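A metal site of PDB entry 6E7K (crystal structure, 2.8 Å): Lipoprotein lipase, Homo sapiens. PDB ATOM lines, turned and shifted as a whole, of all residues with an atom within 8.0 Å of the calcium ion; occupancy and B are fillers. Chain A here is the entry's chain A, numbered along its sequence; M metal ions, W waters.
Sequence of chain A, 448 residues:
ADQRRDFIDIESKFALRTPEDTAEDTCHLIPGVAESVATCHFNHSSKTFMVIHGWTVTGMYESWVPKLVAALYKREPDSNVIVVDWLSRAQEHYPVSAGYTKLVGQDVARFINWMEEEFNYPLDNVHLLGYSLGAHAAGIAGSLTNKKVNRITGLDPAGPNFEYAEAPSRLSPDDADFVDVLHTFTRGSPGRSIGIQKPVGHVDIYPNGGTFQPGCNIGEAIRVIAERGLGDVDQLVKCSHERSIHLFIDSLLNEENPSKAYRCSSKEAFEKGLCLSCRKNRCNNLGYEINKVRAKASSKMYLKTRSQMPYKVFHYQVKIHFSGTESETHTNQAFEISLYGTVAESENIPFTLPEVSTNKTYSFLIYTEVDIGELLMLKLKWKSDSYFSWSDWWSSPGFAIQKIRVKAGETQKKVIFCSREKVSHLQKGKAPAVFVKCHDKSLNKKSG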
ATOM      1  N   HIS A 136      24.770  24.274  -0.586  1.00  0.00           N
ATOM      2  CA  HIS A 136      24.244  23.069   0.018  1.00  0.00           C
ATOM      3  C   HIS A 136      24.788  21.836  -0.719  1.00  0.00           C
ATOM      4  O   HIS A 136      25.063  20.811  -0.098  1.00  0.00           O
ATOM      5  CB  HIS A 136      22.720  23.096   0.063  1.00  0.00           C
ATOM      6  CG  HIS A 136      22.175  24.228   0.856  1.00  0.00           C
ATOM      7  ND1 HIS A 136      22.429  24.365   2.199  1.00  0.00           N
ATOM      8  CD2 HIS A 136      21.420  25.282   0.496  1.00  0.00           C
ATOM      9  CE1 HIS A 136      21.850  25.466   2.643  1.00  0.00           C
ATOM     10  NE2 HIS A 136      21.218  26.047   1.612  1.00  0.00           N
ATOM     11  N   ALA A 138      27.737  21.703  -1.918  1.00  0.00           N
ATOM     12  CA  ALA A 138      29.082  21.670  -1.350  1.00  0.00           C
ATOM     13  C   ALA A 138      29.043  21.098   0.069  1.00  0.00           C
ATOM     14  O   ALA A 138      29.921  20.330   0.478  1.00  0.00           O
ATOM     15  CB  ALA A 138      29.694  23.051  -1.383  1.00  0.00           C
ATOM     16  N   GLY A 139      28.010  21.446   0.836  1.00  0.00           N
ATOM     17  CA  GLY A 139      27.877  20.919   2.193  1.00  0.00           C
ATOM     18  C   GLY A 139      27.725  19.414   2.205  1.00  0.00           C
ATOM     19  O   GLY A 139      28.378  18.722   2.964  1.00  0.00           O
ATOM     20  N   ILE A 140      26.858  18.924   1.320  1.00  0.00           N
ATOM     21  CA  ILE A 140      26.534  17.504   1.222  1.00  0.00           C
ATOM     22  C   ILE A 140      27.771  16.744   0.724  1.00  0.00           C
ATOM     23  O   ILE A 140      28.062  15.643   1.196  1.00  0.00           O
ATOM     24  CB  ILE A 140      25.316  17.301   0.304  1.00  0.00           C
ATOM     25  CG1 ILE A 140      24.089  18.061   0.831  1.00  0.00           C
ATOM     26  CG2 ILE A 140      25.040  15.819   0.112  1.00  0.00           C
ATOM     27  CD1 ILE A 140      22.807  17.824   0.071  1.00  0.00           C
ATOM     28  N   ALA A 141      28.482  17.322  -0.247  1.00  0.00           N
ATOM     29  CA  ALA A 141      29.689  16.714  -0.777  1.00  0.00           C
ATOM     30  C   ALA A 141      30.686  16.529   0.371  1.00  0.00           C
ATOM     31  O   ALA A 141      31.169  15.441   0.629  1.00  0.00           O
ATOM     32  CB  ALA A 141      30.274  17.541  -1.888  1.00  0.00           C
ATOM     33  N   GLY A 142      30.942  17.615   1.094  1.00  0.00           N
ATOM     34  CA  GLY A 142      31.864  17.604   2.215  1.00  0.00           C
ATOM     35  C   GLY A 142      31.516  16.534   3.241  1.00  0.00           C
ATOM     36  O   GLY A 142      32.415  16.038   3.923  1.00  0.00           O
ATOM     37  N   SER A 143      30.229  16.215   3.363  1.00  0.00           N
ATOM     38  CA  SER A 143      29.751  15.244   4.338  1.00  0.00           C
ATOM     39  C   SER A 143      29.925  13.808   3.852  1.00  0.00           C
ATOM     40  O   SER A 143      29.659  12.885   4.592  1.00  0.00           O
ATOM     41  CB  SER A 143      28.306  15.510   4.676  1.00  0.00           C
ATOM     42  OG  SER A 143      27.482  15.352   3.522  1.00  0.00           O
ATOM     43  N   ILE A 152      34.926  24.796   3.407  1.00  0.00           N
ATOM     44  CA  ILE A 152      33.777  25.145   2.564  1.00  0.00           C
ATOM     45  C   ILE A 152      33.427  26.607   2.816  1.00  0.00           C
ATOM     46  O   ILE A 152      33.349  27.048   3.940  1.00  0.00           O
ATOM     47  CB  ILE A 152      32.523  24.259   2.786  1.00  0.00           C
ATOM     48  CG1 ILE A 152      32.784  22.791   2.460  1.00  0.00           C
ATOM     49  CG2 ILE A 152      31.337  24.793   1.985  1.00  0.00           C
ATOM     50  CD1 ILE A 152      31.740  21.850   3.046  1.00  0.00           C
ATOM     51  N   GLU A 166      17.641  19.628   8.241  1.00  0.00           N
ATOM     52  CA  GLU A 166      18.632  19.146   9.180  1.00  0.00           C
ATOM     53  C   GLU A 166      19.958  18.956   8.466  1.00  0.00           C
ATOM     54  O   GLU A 166      20.001  18.849   7.244  1.00  0.00           O
ATOM     55  CB  GLU A 166      18.182  17.844   9.837  1.00  0.00           C
ATOM     56  CG  GLU A 166      17.196  18.097  10.943  1.00  0.00           C
ATOM     57  CD  GLU A 166      16.289  16.911  11.179  1.00  0.00           C
ATOM     58  OE1 GLU A 166      16.642  15.796  10.709  1.00  0.00           O
ATOM     59  OE2 GLU A 166      15.236  17.108  11.804  1.00  0.00           O
ATOM     60  N   ALA A 167      21.028  18.899   9.267  1.00  0.00           N
ATOM     61  CA  ALA A 167      22.379  19.149   8.793  1.00  0.00           C
ATOM     62  C   ALA A 167      22.697  18.251   7.598  1.00  0.00           C
ATOM     63  O   ALA A 167      23.201  18.760   6.605  1.00  0.00           O
ATOM     64  CB  ALA A 167      23.391  18.940   9.899  1.00  0.00           C
ATOM     65  N   PRO A 168      22.379  16.932   7.624  1.00  0.00           N
ATOM     66  CA  PRO A 168      22.708  16.045   6.510  1.00  0.00           C
ATOM     67  C   PRO A 168      22.263  16.590   5.145  1.00  0.00           C
ATOM     68  O   PRO A 168      22.901  16.296   4.128  1.00  0.00           O
ATOM     69  CB  PRO A 168      21.948  14.756   6.837  1.00  0.00           C
ATOM     70  CG  PRO A 168      21.786  14.770   8.331  1.00  0.00           C
ATOM     71  CD  PRO A 168      21.637  16.228   8.698  1.00  0.00           C
ATOM     72  N   SER A 169      21.187  17.400   5.128  1.00  0.00           N
ATOM     73  CA  SER A 169      20.521  17.846   3.910  1.00  0.00           C
ATOM     74  C   SER A 169      20.929  19.268   3.497  1.00  0.00           C
ATOM     75  O   SER A 169      20.496  19.733   2.452  1.00  0.00           O
ATOM     76  CB  SER A 169      19.045  17.750   4.079  1.00  0.00           C
ATOM     77  OG  SER A 169      18.637  16.408   3.868  1.00  0.00           O
ATOM     78  N   ARG A 170      21.764  19.940   4.305  1.00  0.00           N
ATOM     79  CA  ARG A 170      22.220  21.297   3.986  1.00  0.00           C
ATOM     80  C   ARG A 170      23.685  21.485   4.391  1.00  0.00           C
ATOM     81  O   ARG A 170      24.289  20.607   5.027  1.00  0.00           O
ATOM     82  CB  ARG A 170      21.344  22.313   4.743  1.00  0.00           C
ATOM     83  CG  ARG A 170      21.320  22.074   6.239  1.00  0.00           C
ATOM     84  CD  ARG A 170      20.793  23.250   7.014  1.00  0.00           C
ATOM     85  NE  ARG A 170      20.584  22.873   8.403  1.00  0.00           N
ATOM     86  CZ  ARG A 170      21.487  23.019   9.357  1.00  0.00           C
ATOM     87  NH1 ARG A 170      22.650  23.569   9.063  1.00  0.00           N
ATOM     88  NH2 ARG A 170      21.204  22.634  10.582  1.00  0.00           N
ATOM     89  N   LEU A 171      24.234  22.657   4.053  1.00  0.00           N
ATOM     90  CA  LEU A 171      25.505  23.084   4.570  1.00  0.00           C
ATOM     91  C   LEU A 171      25.418  23.165   6.092  1.00  0.00           C
ATOM     92  O   LEU A 171      24.413  23.650   6.654  1.00  0.00           O
ATOM     93  CB  LEU A 171      25.869  24.448   3.969  1.00  0.00           C
ATOM     94  CG  LEU A 171      27.231  24.997   4.393  1.00  0.00           C
ATOM     95  CD1 LEU A 171      28.331  23.982   4.128  1.00  0.00           C
ATOM     96  CD2 LEU A 171      27.522  26.300   3.649  1.00  0.00           C
ATOM     97  N   SER A 172      26.450  22.661   6.765  1.00  0.00           N
ATOM     98  CA  SER A 172      26.506  22.737   8.199  1.00  0.00           C
ATOM     99  C   SER A 172      27.958  22.681   8.632  1.00  0.00           C
ATOM    100  O   SER A 172      28.828  22.326   7.844  1.00  0.00           O
ATOM    101  CB  SER A 172      25.668  21.655   8.834  1.00  0.00           C
ATOM    102  OG  SER A 172      26.242  20.368   8.616  1.00  0.00           O
ATOM    103  N   PRO A 173      28.280  23.065   9.887  1.00  0.00           N
ATOM    104  CA  PRO A 173      29.675  23.170  10.306  1.00  0.00           C
ATOM    105  C   PRO A 173      30.442  21.844  10.253  1.00  0.00           C
ATOM    106  O   PRO A 173      31.645  21.856  10.122  1.00  0.00           O
ATOM    107  CB  PRO A 173      29.554  23.727  11.731  1.00  0.00           C
ATOM    108  CG  PRO A 173      28.204  24.420  11.725  1.00  0.00           C
ATOM    109  CD  PRO A 173      27.333  23.486  10.926  1.00  0.00           C
ATOM    110  N   ASP A 174      29.733  20.709  10.344  1.00  0.00           N
ATOM    111  CA  ASP A 174      30.372  19.406  10.368  1.00  0.00           C
ATOM    112  C   ASP A 174      30.931  19.048   8.981  1.00  0.00           C
ATOM    113  O   ASP A 174      31.716  18.105   8.862  1.00  0.00           O
ATOM    114  CB  ASP A 174      29.425  18.318  10.898  1.00  0.00           C
ATOM    115  CG  ASP A 174      28.154  18.061  10.085  1.00  0.00           C
ATOM    116  OD1 ASP A 174      28.164  18.168   8.839  1.00  0.00           O
ATOM    117  OD2 ASP A 174      27.139  17.679  10.712  1.00  0.00           O
ATOM    118  N   ASP A 175      30.550  19.794   7.918  1.00  0.00           N
ATOM    119  CA  ASP A 175      30.740  19.339   6.536  1.00  0.00           C
ATOM    120  C   ASP A 175      32.190  19.552   6.059  1.00  0.00           C
ATOM    121  O   ASP A 175      32.604  18.993   5.034  1.00  0.00           O
ATOM    122  CB  ASP A 175      29.716  20.001   5.602  1.00  0.00           C
ATOM    123  CG  ASP A 175      28.299  19.503   5.832  1.00  0.00           C
ATOM    124  OD1 ASP A 175      28.131  18.404   6.430  1.00  0.00           O
ATOM    125  OD2 ASP A 175      27.377  20.218   5.427  1.00  0.00           O
ATOM    126  N   ALA A 176      32.956  20.353   6.796  1.00  0.00           N
ATOM    127  CA  ALA A 176      34.360  20.540   6.514  1.00  0.00           C
ATOM    128  C   ALA A 176      35.103  20.852   7.818  1.00  0.00           C
ATOM    129  O   ALA A 176      34.479  21.075   8.852  1.00  0.00           O
ATOM    130  CB  ALA A 176      34.530  21.631   5.474  1.00  0.00           C
ATOM    131  N   VAL A 200      25.025  28.586   9.544  1.00  0.00           N
ATOM    132  CA  VAL A 200      25.300  27.201   9.157  1.00  0.00           C
ATOM    133  C   VAL A 200      26.823  26.945   9.058  1.00  0.00           C
ATOM    134  O   VAL A 200      27.260  25.908   8.565  1.00  0.00           O
ATOM    135  CB  VAL A 200      24.567  26.858   7.854  1.00  0.00           C
ATOM    136  CG1 VAL A 200      23.061  26.991   8.018  1.00  0.00           C
ATOM    137  CG2 VAL A 200      25.049  27.707   6.677  1.00  0.00           C
HETATM  138 CA    CA M   1      25.560  18.844   6.546  1.00  0.00          CA
HETATM  139  O   HOH W   1      26.169  16.981   7.941  1.00  0.00           O
HETATM  140  O   HOH W   2      25.512  17.877   4.294  1.00  0.00           O
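Merely in contact with the calcium ion: Asp 174 (3.5 Å) and Pro 168 (3.9 Å). Within 4 Å of the calcium ion: Ala 167, Pro 168, Arg 170, Ser 172, Asp 174 and Asp 175.
O of Ala 167 binds the calcium ion (2.4 Å). Water W1 is bound to the calcium ion (2.4 Å). The calcium ion is bound by water W2. OD2 of Asp 175 binds the calcium ion. The calcium ion is bound by OD1 of Asp 175 (2.6 Å). The calcium ion is bound by O of Arg 170. The side-chain hydroxyl (OG) of Ser 172 binds the calcium ion (2.7 Å). The calcium ion has seven donor atoms within binding distance.
Water W2 lies within hydrogen-bond range of the backbone carbonyl oxygen of Pro 168 (3.1 Å), the backbone carbonyl oxygen of Gly 139 (3.3 Å), the side-chain hydroxyl of Ser 143 (3.3 Å) and the backbone NH of Ile 140 (3.4 Å).
OD1 of Asp 174 lies close to OD1 of Asp 175 (2.4 Å). OG of Ser 172 lies close to OD1 of Asp 174 (2.9 Å).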
